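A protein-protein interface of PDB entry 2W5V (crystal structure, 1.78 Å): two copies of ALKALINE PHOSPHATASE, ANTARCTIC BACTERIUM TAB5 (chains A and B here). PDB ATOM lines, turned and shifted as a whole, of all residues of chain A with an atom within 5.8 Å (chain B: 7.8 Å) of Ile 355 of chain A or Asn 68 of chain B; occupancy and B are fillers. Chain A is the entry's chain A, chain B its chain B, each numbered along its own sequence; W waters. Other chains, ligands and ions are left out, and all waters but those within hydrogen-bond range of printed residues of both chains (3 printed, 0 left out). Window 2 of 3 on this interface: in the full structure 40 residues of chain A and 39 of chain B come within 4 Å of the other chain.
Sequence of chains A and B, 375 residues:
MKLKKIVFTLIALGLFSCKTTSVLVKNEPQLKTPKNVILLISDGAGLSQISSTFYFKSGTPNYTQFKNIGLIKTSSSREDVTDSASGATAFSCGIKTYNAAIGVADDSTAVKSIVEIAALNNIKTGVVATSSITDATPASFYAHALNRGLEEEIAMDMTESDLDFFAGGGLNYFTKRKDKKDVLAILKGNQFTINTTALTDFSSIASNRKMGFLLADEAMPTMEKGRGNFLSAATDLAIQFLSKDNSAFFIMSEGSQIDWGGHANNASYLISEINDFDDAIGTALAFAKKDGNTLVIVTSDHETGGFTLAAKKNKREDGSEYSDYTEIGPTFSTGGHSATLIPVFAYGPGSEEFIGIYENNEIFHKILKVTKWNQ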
ATOM      1  N   ASN A  68       0.192   2.003  -3.794  1.00  0.00           N
ATOM      2  CA  ASN A  68       0.108   3.307  -4.432  1.00  0.00           C
ATOM      3  C   ASN A  68       1.361   4.128  -4.188  1.00  0.00           C
ATOM      4  O   ASN A  68       1.706   4.450  -3.045  1.00  0.00           O
ATOM      5  CB  ASN A  68      -1.132   4.063  -3.965  1.00  0.00           C
ATOM      6  CG  ASN A  68      -2.408   3.351  -4.359  1.00  0.00           C
ATOM      7  OD1 ASN A  68      -2.587   2.983  -5.522  1.00  0.00           O
ATOM      8  ND2 ASN A  68      -3.290   3.133  -3.394  1.00  0.00           N
ATOM      9  N   ILE A  69       2.034   4.453  -5.283  1.00  0.00           N
ATOM     10  CA  ILE A  69       3.317   5.137  -5.233  1.00  0.00           C
ATOM     11  C   ILE A  69       3.302   6.323  -6.183  1.00  0.00           C
ATOM     12  O   ILE A  69       2.812   6.219  -7.307  1.00  0.00           O
ATOM     13  CB  ILE A  69       4.475   4.167  -5.590  1.00  0.00           C
ATOM     14  CG1 ILE A  69       4.548   3.038  -4.551  1.00  0.00           C
ATOM     15  CG2 ILE A  69       5.794   4.916  -5.653  1.00  0.00           C
ATOM     16  CD1 ILE A  69       5.415   1.848  -4.955  1.00  0.00           C
ATOM     17  N   GLY A  70       3.835   7.447  -5.722  1.00  0.00           N
ATOM     18  CA  GLY A  70       3.979   8.623  -6.559  1.00  0.00           C
ATOM     19  C   GLY A  70       5.387   9.165  -6.446  1.00  0.00           C
ATOM     20  O   GLY A  70       6.225   8.572  -5.762  1.00  0.00           O
ATOM     21  N   LEU A  71       5.652  10.282  -7.113  1.00  0.00           N
ATOM     22  CA  LEU A  71       6.959  10.930  -7.033  1.00  0.00           C
ATOM     23  C   LEU A  71       6.764  12.437  -6.920  1.00  0.00           C
ATOM     24  O   LEU A  71       5.918  13.007  -7.619  1.00  0.00           O
ATOM     25  CB  LEU A  71       7.799  10.632  -8.289  1.00  0.00           C
ATOM     26  CG  LEU A  71       8.164   9.188  -8.613  1.00  0.00           C
ATOM     27  CD1 LEU A  71       8.617   9.095 -10.063  1.00  0.00           C
ATOM     28  CD2 LEU A  71       9.239   8.664  -7.667  1.00  0.00           C
ATOM     29  N   SER A 351      -5.762   6.840  -0.877  1.00  0.00           N
ATOM     30  CA  SER A 351      -4.341   6.656  -1.176  1.00  0.00           C
ATOM     31  C   SER A 351      -4.029   6.819  -2.672  1.00  0.00           C
ATOM     32  O   SER A 351      -2.914   7.209  -3.040  1.00  0.00           O
ATOM     33  CB  SER A 351      -3.844   5.297  -0.670  1.00  0.00           C
ATOM     34  OG  SER A 351      -4.524   4.241  -1.331  1.00  0.00           O
ATOM     35  N   GLU A 352      -5.015   6.543  -3.526  1.00  0.00           N
ATOM     36  CA  GLU A 352      -4.817   6.643  -4.980  1.00  0.00           C
ATOM     37  C   GLU A 352      -4.616   8.089  -5.466  1.00  0.00           C
ATOM     38  O   GLU A 352      -4.151   8.327  -6.581  1.00  0.00           O
ATOM     39  CB  GLU A 352      -5.985   5.984  -5.712  1.00  0.00           C
ATOM     40  CG  GLU A 352      -5.942   4.459  -5.621  1.00  0.00           C
ATOM     41  CD  GLU A 352      -7.300   3.800  -5.790  1.00  0.00           C
ATOM     42  OE1 GLU A 352      -7.723   3.080  -4.860  1.00  0.00           O
ATOM     43  OE2 GLU A 352      -7.941   3.995  -6.846  1.00  0.00           O
ATOM     44  N   GLU A 353      -4.988   9.054  -4.634  1.00  0.00           N
ATOM     45  CA  GLU A 353      -4.812  10.464  -4.972  1.00  0.00           C
ATOM     46  C   GLU A 353      -3.331  10.832  -5.031  1.00  0.00           C
ATOM     47  O   GLU A 353      -2.961  11.888  -5.558  1.00  0.00           O
ATOM     48  CB  GLU A 353      -5.504  11.343  -3.925  1.00  0.00           C
ATOM     49  CG  GLU A 353      -5.766  12.758  -4.401  1.00  0.00           C
ATOM     50  CD  GLU A 353      -6.736  12.775  -5.570  1.00  0.00           C
ATOM     51  OE1 GLU A 353      -7.672  11.946  -5.579  1.00  0.00           O
ATOM     52  OE2 GLU A 353      -6.556  13.603  -6.482  1.00  0.00           O
ATOM     53  N   PHE A 354      -2.484   9.961  -4.494  1.00  0.00           N
ATOM     54  CA  PHE A 354      -1.064  10.285  -4.312  1.00  0.00           C
ATOM     55  C   PHE A 354      -0.109   9.704  -5.364  1.00  0.00           C
ATOM     56  O   PHE A 354       1.112   9.813  -5.231  1.00  0.00           O
ATOM     57  CB  PHE A 354      -0.629   9.908  -2.889  1.00  0.00           C
ATOM     58  CG  PHE A 354      -1.295  10.749  -1.835  1.00  0.00           C
ATOM     59  CD1 PHE A 354      -2.564  10.429  -1.364  1.00  0.00           C
ATOM     60  CD2 PHE A 354      -0.687  11.903  -1.374  1.00  0.00           C
ATOM     61  CE1 PHE A 354      -3.197  11.235  -0.415  1.00  0.00           C
ATOM     62  CE2 PHE A 354      -1.309  12.708  -0.431  1.00  0.00           C
ATOM     63  CZ  PHE A 354      -2.566  12.379   0.048  1.00  0.00           C
ATOM     64  N   ILE A 355      -0.668   9.112  -6.414  1.00  0.00           N
ATOM     65  CA  ILE A 355       0.142   8.534  -7.478  1.00  0.00           C
ATOM     66  C   ILE A 355       0.524   9.582  -8.523  1.00  0.00           C
ATOM     67  O   ILE A 355       0.194  10.759  -8.382  1.00  0.00           O
ATOM     68  CB  ILE A 355      -0.564   7.318  -8.124  1.00  0.00           C
ATOM     69  CG1 ILE A 355      -1.809   7.736  -8.917  1.00  0.00           C
ATOM     70  CG2 ILE A 355      -0.938   6.292  -7.052  1.00  0.00           C
ATOM     71  CD1 ILE A 355      -2.442   6.558  -9.705  1.00  0.00           C
ATOM     72  N   GLY A 356       1.237   9.163  -9.562  1.00  0.00           N
ATOM     73  CA  GLY A 356       1.749  10.097 -10.545  1.00  0.00           C
ATOM     74  C   GLY A 356       2.893  10.953 -10.017  1.00  0.00           C
ATOM     75  O   GLY A 356       3.475  10.668  -8.972  1.00  0.00           O
ATOM     76  N   ILE A 357       3.211  12.008 -10.756  1.00  0.00           N
ATOM     77  CA  ILE A 357       4.363  12.861 -10.470  1.00  0.00           C
ATOM     78  C   ILE A 357       3.847  14.273 -10.263  1.00  0.00           C
ATOM     79  O   ILE A 357       3.070  14.766 -11.072  1.00  0.00           O
ATOM     80  CB  ILE A 357       5.351  12.854 -11.656  1.00  0.00           C
ATOM     81  CG1 ILE A 357       5.734  11.414 -11.996  1.00  0.00           C
ATOM     82  CG2 ILE A 357       6.592  13.676 -11.335  1.00  0.00           C
ATOM     83  CD1 ILE A 357       6.780  11.301 -13.083  1.00  0.00           C
ATOM     84  N   TYR A 358       4.262  14.920  -9.179  1.00  0.00           N
ATOM     85  CA  TYR A 358       3.749  16.258  -8.859  1.00  0.00           C
ATOM     86  C   TYR A 358       4.750  17.033  -8.014  1.00  0.00           C
ATOM     87  O   TYR A 358       5.747  16.473  -7.565  1.00  0.00           O
ATOM     88  CB  TYR A 358       2.391  16.174  -8.145  1.00  0.00           C
ATOM     89  CG  TYR A 358       2.286  15.094  -7.076  1.00  0.00           C
ATOM     90  CD1 TYR A 358       2.489  15.403  -5.727  1.00  0.00           C
ATOM     91  CD2 TYR A 358       1.970  13.771  -7.412  1.00  0.00           C
ATOM     92  CE1 TYR A 358       2.388  14.429  -4.741  1.00  0.00           C
ATOM     93  CE2 TYR A 358       1.875  12.790  -6.435  1.00  0.00           C
ATOM     94  CZ  TYR A 358       2.083  13.129  -5.096  1.00  0.00           C
ATOM     95  OH  TYR A 358       1.985  12.172  -4.102  1.00  0.00           O
ATOM     96  N   LYS A 366      -3.499  17.548  -1.674  1.00  0.00           N
ATOM     97  CA  LYS A 366      -4.062  16.204  -1.794  1.00  0.00           C
ATOM     98  C   LYS A 366      -4.635  15.705  -0.463  1.00  0.00           C
ATOM     99  O   LYS A 366      -5.683  15.054  -0.438  1.00  0.00           O
ATOM    100  CB  LYS A 366      -3.020  15.232  -2.364  1.00  0.00           C
ATOM    101  CG  LYS A 366      -2.668  15.507  -3.819  1.00  0.00           C
ATOM    102  CD  LYS A 366      -1.432  14.714  -4.261  1.00  0.00           C
ATOM    103  CE  LYS A 366      -1.113  14.952  -5.732  1.00  0.00           C
ATOM    104  NZ  LYS A 366      -2.200  14.464  -6.615  1.00  0.00           N
ATOM    105  N   GLN B  65       3.462  12.067 -17.733  1.00  0.00           N
ATOM    106  CA  GLN B  65       2.200  11.494 -18.197  1.00  0.00           C
ATOM    107  C   GLN B  65       1.784  10.259 -17.397  1.00  0.00           C
ATOM    108  O   GLN B  65       0.626   9.854 -17.446  1.00  0.00           O
ATOM    109  CB  GLN B  65       2.280  11.133 -19.682  1.00  0.00           C
ATOM    110  CG  GLN B  65       2.489  12.312 -20.608  1.00  0.00           C
ATOM    111  CD  GLN B  65       2.401  11.930 -22.072  1.00  0.00           C
ATOM    112  OE1 GLN B  65       1.407  11.352 -22.517  1.00  0.00           O
ATOM    113  NE2 GLN B  65       3.439  12.257 -22.834  1.00  0.00           N
ATOM    114  N   PHE B  66       2.721   9.649 -16.671  1.00  0.00           N
ATOM    115  CA  PHE B  66       2.425   8.396 -15.975  1.00  0.00           C
ATOM    116  C   PHE B  66       1.771   8.600 -14.616  1.00  0.00           C
ATOM    117  O   PHE B  66       2.146   9.496 -13.866  1.00  0.00           O
ATOM    118  CB  PHE B  66       3.692   7.552 -15.784  1.00  0.00           C
ATOM    119  CG  PHE B  66       4.228   6.953 -17.051  1.00  0.00           C
ATOM    120  CD1 PHE B  66       5.309   7.531 -17.707  1.00  0.00           C
ATOM    121  CD2 PHE B  66       3.668   5.799 -17.581  1.00  0.00           C
ATOM    122  CE1 PHE B  66       5.804   6.974 -18.870  1.00  0.00           C
ATOM    123  CE2 PHE B  66       4.166   5.235 -18.746  1.00  0.00           C
ATOM    124  CZ  PHE B  66       5.230   5.822 -19.386  1.00  0.00           C
ATOM    125  N   LYS B  67       0.801   7.751 -14.301  1.00  0.00           N
ATOM    126  CA  LYS B  67       0.169   7.758 -12.990  1.00  0.00           C
ATOM    127  C   LYS B  67       0.578   6.505 -12.216  1.00  0.00           C
ATOM    128  O   LYS B  67       0.975   6.570 -11.046  1.00  0.00           O
ATOM    129  CB  LYS B  67      -1.355   7.805 -13.139  1.00  0.00           C
ATOM    130  CG  LYS B  67      -1.863   9.050 -13.836  1.00  0.00           C
ATOM    131  CD  LYS B  67      -1.354  10.293 -13.118  1.00  0.00           C
ATOM    132  CE  LYS B  67      -1.778  11.574 -13.805  1.00  0.00           C
ATOM    133  NZ  LYS B  67      -1.232  12.770 -13.087  1.00  0.00           N
ATOM    134  N   ASN B  68       0.471   5.357 -12.877  1.00  0.00           N
ATOM    135  CA  ASN B  68       0.797   4.080 -12.254  1.00  0.00           C
ATOM    136  C   ASN B  68       2.303   3.863 -12.194  1.00  0.00           C
ATOM    137  O   ASN B  68       2.960   3.789 -13.232  1.00  0.00           O
ATOM    138  CB  ASN B  68       0.127   2.944 -13.021  1.00  0.00           C
ATOM    139  CG  ASN B  68      -1.384   3.044 -12.988  1.00  0.00           C
ATOM    140  OD1 ASN B  68      -1.968   3.359 -11.948  1.00  0.00           O
ATOM    141  ND2 ASN B  68      -2.027   2.786 -14.123  1.00  0.00           N
ATOM    142  N   ILE B  69       2.831   3.767 -10.976  1.00  0.00           N
ATOM    143  CA  ILE B  69       4.268   3.672 -10.738  1.00  0.00           C
ATOM    144  C   ILE B  69       4.564   2.553  -9.753  1.00  0.00           C
ATOM    145  O   ILE B  69       3.837   2.382  -8.767  1.00  0.00           O
ATOM    146  CB  ILE B  69       4.800   5.011 -10.166  1.00  0.00           C
ATOM    147  CG1 ILE B  69       4.673   6.110 -11.219  1.00  0.00           C
ATOM    148  CG2 ILE B  69       6.240   4.862  -9.680  1.00  0.00           C
ATOM    149  CD1 ILE B  69       4.811   7.538 -10.674  1.00  0.00           C
ATOM    150  N   GLY B  70       5.605   1.765 -10.030  1.00  0.00           N
ATOM    151  CA  GLY B  70       6.036   0.710  -9.123  1.00  0.00           C
ATOM    152  C   GLY B  70       7.542   0.777  -8.913  1.00  0.00           C
ATOM    153  O   GLY B  70       8.181   1.696  -9.409  1.00  0.00           O
ATOM    154  N   LEU B 295      -0.394  -1.170 -24.012  1.00  0.00           N
ATOM    155  CA  LEU B 295       0.238  -0.985 -22.713  1.00  0.00           C
ATOM    156  C   LEU B 295       1.682  -0.546 -22.912  1.00  0.00           C
ATOM    157  O   LEU B 295       2.448  -1.198 -23.617  1.00  0.00           O
ATOM    158  CB  LEU B 295       0.196  -2.292 -21.922  1.00  0.00           C
ATOM    159  CG  LEU B 295       1.093  -2.370 -20.687  1.00  0.00           C
ATOM    160  CD1 LEU B 295       0.536  -1.498 -19.553  1.00  0.00           C
ATOM    161  CD2 LEU B 295       1.266  -3.815 -20.233  1.00  0.00           C
ATOM    162  N   VAL B 296       2.050   0.567 -22.298  1.00  0.00           N
ATOM    163  CA  VAL B 296       3.421   1.047 -22.362  1.00  0.00           C
ATOM    164  C   VAL B 296       4.057   0.920 -20.990  1.00  0.00           C
ATOM    165  O   VAL B 296       3.541   1.454 -20.008  1.00  0.00           O
ATOM    166  CB  VAL B 296       3.479   2.517 -22.789  1.00  0.00           C
ATOM    167  CG1 VAL B 296       4.919   2.994 -22.812  1.00  0.00           C
ATOM    168  CG2 VAL B 296       2.812   2.717 -24.153  1.00  0.00           C
ATOM    169  N   VAL B 298       7.707   1.434 -18.884  1.00  0.00           N
ATOM    170  CA  VAL B 298       9.031   2.057 -18.890  1.00  0.00           C
ATOM    171  C   VAL B 298       9.763   1.695 -17.607  1.00  0.00           C
ATOM    172  O   VAL B 298       9.239   1.899 -16.502  1.00  0.00           O
ATOM    173  CB  VAL B 298       8.946   3.596 -18.957  1.00  0.00           C
ATOM    174  CG1 VAL B 298      10.342   4.197 -18.850  1.00  0.00           C
ATOM    175  CG2 VAL B 298       8.258   4.061 -20.251  1.00  0.00           C
ATOM    176  N   VAL B 344       9.304   1.805 -12.016  1.00  0.00           N
ATOM    177  CA  VAL B 344       8.604   1.263 -13.164  1.00  0.00           C
ATOM    178  C   VAL B 344       7.420   2.176 -13.422  1.00  0.00           C
ATOM    179  O   VAL B 344       6.698   2.540 -12.487  1.00  0.00           O
ATOM    180  CB  VAL B 344       8.031  -0.124 -12.844  1.00  0.00           C
ATOM    181  CG1 VAL B 344       7.160  -0.634 -14.003  1.00  0.00           C
ATOM    182  CG2 VAL B 344       9.158  -1.095 -12.497  1.00  0.00           C
ATOM    183  N   PHE B 345       7.222   2.548 -14.685  1.00  0.00           N
ATOM    184  CA  PHE B 345       6.091   3.376 -15.086  1.00  0.00           C
ATOM    185  C   PHE B 345       5.238   2.590 -16.073  1.00  0.00           C
ATOM    186  O   PHE B 345       5.770   1.933 -16.970  1.00  0.00           O
ATOM    187  CB  PHE B 345       6.570   4.669 -15.756  1.00  0.00           C
ATOM    188  CG  PHE B 345       7.526   5.484 -14.922  1.00  0.00           C
ATOM    189  CD1 PHE B 345       7.058   6.495 -14.086  1.00  0.00           C
ATOM    190  CD2 PHE B 345       8.891   5.260 -14.990  1.00  0.00           C
ATOM    191  CE1 PHE B 345       7.934   7.253 -13.315  1.00  0.00           C
ATOM    192  CE2 PHE B 345       9.779   6.019 -14.230  1.00  0.00           C
ATOM    193  CZ  PHE B 345       9.294   7.027 -13.388  1.00  0.00           C
ATOM    194  N   ALA B 346       3.918   2.655 -15.925  1.00  0.00           N
ATOM    195  CA  ALA B 346       3.039   1.955 -16.863  1.00  0.00           C
ATOM    196  C   ALA B 346       1.802   2.770 -17.224  1.00  0.00           C
ATOM    197  O   ALA B 346       1.167   3.369 -16.365  1.00  0.00           O
ATOM    198  CB  ALA B 346       2.635   0.588 -16.308  1.00  0.00           C
ATOM    199  N   TYR B 347       1.461   2.764 -18.506  1.00  0.00           N
ATOM    200  CA  TYR B 347       0.292   3.470 -19.003  1.00  0.00           C
ATOM    201  C   TYR B 347      -0.505   2.543 -19.910  1.00  0.00           C
ATOM    202  O   TYR B 347       0.076   1.839 -20.733  1.00  0.00           O
ATOM    203  CB  TYR B 347       0.702   4.696 -19.822  1.00  0.00           C
ATOM    204  CG  TYR B 347      -0.503   5.363 -20.446  1.00  0.00           C
ATOM    205  CD1 TYR B 347      -1.194   6.353 -19.766  1.00  0.00           C
ATOM    206  CD2 TYR B 347      -0.979   4.962 -21.690  1.00  0.00           C
ATOM    207  CE1 TYR B 347      -2.312   6.947 -20.318  1.00  0.00           C
ATOM    208  CE2 TYR B 347      -2.100   5.549 -22.249  1.00  0.00           C
ATOM    209  CZ  TYR B 347      -2.762   6.540 -21.560  1.00  0.00           C
ATOM    210  OH  TYR B 347      -3.878   7.134 -22.107  1.00  0.00           O
ATOM    211  N   GLY B 348      -1.828   2.567 -19.787  1.00  0.00           N
ATOM    212  CA  GLY B 348      -2.680   1.825 -20.700  1.00  0.00           C
ATOM    213  C   GLY B 348      -3.371   0.651 -20.029  1.00  0.00           C
ATOM    214  O   GLY B 348      -3.274   0.482 -18.814  1.00  0.00           O
ATOM    215  N   PRO B 349      -4.086  -0.162 -20.818  1.00  0.00           N
ATOM    216  CA  PRO B 349      -4.821  -1.323 -20.303  1.00  0.00           C
ATOM    217  C   PRO B 349      -3.899  -2.261 -19.544  1.00  0.00           C
ATOM    218  O   PRO B 349      -2.886  -2.686 -20.097  1.00  0.00           O
ATOM    219  CB  PRO B 349      -5.320  -2.017 -21.575  1.00  0.00           C
ATOM    220  CG  PRO B 349      -5.361  -0.965 -22.605  1.00  0.00           C
ATOM    221  CD  PRO B 349      -4.272   0.021 -22.268  1.00  0.00           C
ATOM    222  N   GLY B 350      -4.240  -2.571 -18.297  1.00  0.00           N
ATOM    223  CA  GLY B 350      -3.435  -3.457 -17.477  1.00  0.00           C
ATOM    224  C   GLY B 350      -2.324  -2.769 -16.697  1.00  0.00           C
ATOM    225  O   GLY B 350      -1.608  -3.412 -15.921  1.00  0.00           O
ATOM    226  N   SER B 351      -2.170  -1.466 -16.887  1.00  0.00           N
ATOM    227  CA  SER B 351      -1.034  -0.761 -16.288  1.00  0.00           C
ATOM    228  C   SER B 351      -1.051  -0.811 -14.752  1.00  0.00           C
ATOM    229  O   SER B 351      -0.003  -0.712 -14.112  1.00  0.00           O
ATOM    230  CB  SER B 351      -0.951   0.690 -16.793  1.00  0.00           C
ATOM    231  OG  SER B 351      -2.133   1.416 -16.488  1.00  0.00           O
ATOM    232  N   GLU B 352      -2.231  -0.988 -14.164  1.00  0.00           N
ATOM    233  CA  GLU B 352      -2.353  -1.022 -12.704  1.00  0.00           C
ATOM    234  C   GLU B 352      -1.632  -2.240 -12.106  1.00  0.00           C
ATOM    235  O   GLU B 352      -1.279  -2.248 -10.935  1.00  0.00           O
ATOM    236  CB  GLU B 352      -3.825  -1.038 -12.274  1.00  0.00           C
ATOM    237  CG  GLU B 352      -4.625   0.219 -12.626  1.00  0.00           C
ATOM    238  CD  GLU B 352      -5.011   0.319 -14.106  1.00  0.00           C
ATOM    239  OE1 GLU B 352      -4.798  -0.648 -14.882  1.00  0.00           O
ATOM    240  OE2 GLU B 352      -5.540   1.385 -14.492  1.00  0.00           O
ATOM    241  N   GLU B 353      -1.433  -3.274 -12.916  1.00  0.00           N
ATOM    242  CA  GLU B 353      -0.750  -4.474 -12.445  1.00  0.00           C
ATOM    243  C   GLU B 353       0.690  -4.188 -12.019  1.00  0.00           C
ATOM    244  O   GLU B 353       1.282  -4.949 -11.247  1.00  0.00           O
ATOM    245  CB  GLU B 353      -0.766  -5.551 -13.535  1.00  0.00           C
ATOM    246  CG  GLU B 353      -0.154  -6.873 -13.101  1.00  0.00           C
ATOM    247  CD  GLU B 353      -0.905  -7.512 -11.942  1.00  0.00           C
ATOM    248  OE1 GLU B 353      -2.149  -7.405 -11.908  1.00  0.00           O
ATOM    249  OE2 GLU B 353      -0.249  -8.125 -11.068  1.00  0.00           O
ATOM    250  N   PHE B 354       1.248  -3.079 -12.498  1.00  0.00           N
ATOM    251  CA  PHE B 354       2.674  -2.820 -12.298  1.00  0.00           C
ATOM    252  C   PHE B 354       3.021  -1.916 -11.108  1.00  0.00           C
ATOM    253  O   PHE B 354       4.174  -1.499 -10.974  1.00  0.00           O
ATOM    254  CB  PHE B 354       3.293  -2.273 -13.590  1.00  0.00           C
ATOM    255  CG  PHE B 354       3.239  -3.249 -14.724  1.00  0.00           C
ATOM    256  CD1 PHE B 354       2.071  -3.416 -15.455  1.00  0.00           C
ATOM    257  CD2 PHE B 354       4.334  -4.049 -15.021  1.00  0.00           C
ATOM    258  CE1 PHE B 354       2.004  -4.340 -16.488  1.00  0.00           C
ATOM    259  CE2 PHE B 354       4.272  -4.980 -16.050  1.00  0.00           C
ATOM    260  CZ  PHE B 354       3.105  -5.130 -16.776  1.00  0.00           C
ATOM    261  N   ILE B 355       2.053  -1.634 -10.237  1.00  0.00           N
ATOM    262  CA  ILE B 355       2.322  -0.788  -9.065  1.00  0.00           C
ATOM    263  C   ILE B 355       2.888  -1.609  -7.904  1.00  0.00           C
ATOM    264  O   ILE B 355       3.093  -2.811  -8.032  1.00  0.00           O
ATOM    265  CB  ILE B 355       1.073  -0.005  -8.617  1.00  0.00           C
ATOM    266  CG1 ILE B 355      -0.005  -0.947  -8.073  1.00  0.00           C
ATOM    267  CG2 ILE B 355       0.530   0.847  -9.773  1.00  0.00           C
ATOM    268  CD1 ILE B 355      -1.280  -0.218  -7.654  1.00  0.00           C
ATOM    269  N   GLY B 356       3.158  -0.969  -6.774  1.00  0.00           N
ATOM    270  CA  GLY B 356       3.781  -1.673  -5.667  1.00  0.00           C
ATOM    271  C   GLY B 356       5.255  -1.989  -5.896  1.00  0.00           C
ATOM    272  O   GLY B 356       5.900  -1.449  -6.804  1.00  0.00           O
HETATM  273  O   HOH W   1       0.415  14.423 -11.303  1.00  0.00           O
HETATM  274  O   HOH W   2       1.628   3.928  -8.174  1.00  0.00           O
HETATM  275  O   HOH W   3       1.946  12.141 -13.364  1.00  0.00           O
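The backbone NH (N) of Gly 356 of chain A is in hydrogen-bond range of the backbone carbonyl oxygen (O) of Lys 67 of chain B (3.0 Å).
The backbone NH (N) of Leu 71 of chain A lies within hydrogen-bond range of the backbone carbonyl oxygen (O) of Gly 356 of chain A, 2.9 Å away. The backbone NH (N) of Tyr 358 of chain A is in hydrogen-bond range of the backbone carbonyl oxygen (O) of Leu 71 of chain A (3.0 Å). The backbone carbonyl oxygen of Asn 68 of chain B lies within hydrogen-bond range of the backbone NH of Ala 346 of chain B (3.1 Å). The side-chain amide nitrogen (ND2) of Asn 68 of chain B sits at hydrogen-bond distance from the side-chain hydroxyl (OG) of Ser 351 of chain B (2.7 Å). The backbone carbonyl oxygen (O) of Phe 345 of chain B lies within hydrogen-bond range of the backbone NH (N) of Val 298 of chain B.
Among the printed residues, merely in contact across the chains: Ile 69 of chain A with Ile 69 of chain B, Ile 69 of chain A with Gly 356 of chain B, Leu 71 of chain A with Phe 345 of chain B, Ile 355 of chain A with Lys 67 of chain B, Ile 355 of chain A with Asn 68 of chain B, Gly 356 of chain A with Phe 66 of chain B and Gly 356 of chain A with Ile 69 of chain B.
Of chain B, only Lys 67 (3.4 Å) and Asn 68 (3.9 Å) come within 4 Å of Ile 355 of chain A. Asn 68 of chain B touches one residue of chain A. Of the printed residues of chain A, Phe 345 of chain B touches Leu 71 (3.8 Å). Printed residues of chain A within 4 Å of Ile 69 of chain B: Ile 69 and Gly 356. Of the printed residues of chain A, Phe 66 of chain B touches Gly 356 (3.4 Å). Of the printed residues of chain A, Lys 67 of chain B touches Ile 355 (3.4 Å) and Gly 356 (3.0 Å). Lys 366 of chain A touches none of the printed residues of chain B. The nearest residue of chain A that does not touch Asn 68 of chain B is Gly 356 of chain A (5.1 Å). The nearest printed residue of chain B that does not touch Ile 69 of chain A is Lys 67 of chain B (4.2 Å).
Hydrophobic or aromatic side chains of chain B that line the printed part of chain A: Ile 69 and Phe 345. Along chain B the printed residues that touch a printed residue of chain A span positions 66 to 356. Hydrophobic or aromatic side chains of chain A that line the printed part of chain B: Ile 69, Leu 71 and Ile 355. Among the printed residues, 8 pairs touch across the chains. Among the printed residues, no Asp or Glu carboxylate lies within 4 Å of a Lys or Arg side-chain nitrogen of the other chain.
Ile 69 of chain A touches its own counterpart, Ile 69 of chain B. Ile 69 of chain A touches Gly 356 of chain B, and with the chains exchanged Gly 356 of chain A touches Ile 69 of chain B. Ile 355 of chain A touches Asn 68 of chain B, but with the chains exchanged Asn 68 of chain A does not touch Ile 355 of chain B (4.1 Å). Positions printed for both chains: 68, 69, 70, 351, 352, 353, 354, 355 and 356.
Water W1 lies within hydrogen-bond range of the backbone carbonyl oxygen of Ile 357 of chain A (2.7 Å) and the side-chain amino group of Lys 67 of chain B (2.9 Å). Water W3 lies within hydrogen-bond range of the backbone carbonyl oxygen (O) of Phe 66 of chain B, the backbone NH (N) of Ile 357 of chain A and the side-chain amino group (NZ) of Lys 67 of chain B. Water W2 lies within hydrogen-bond range of the backbone carbonyl oxygen (O) of Ile 69 of chain A (2.7 Å) and the backbone carbonyl oxygen (O) of Ile 69 of chain B (2.8 Å).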
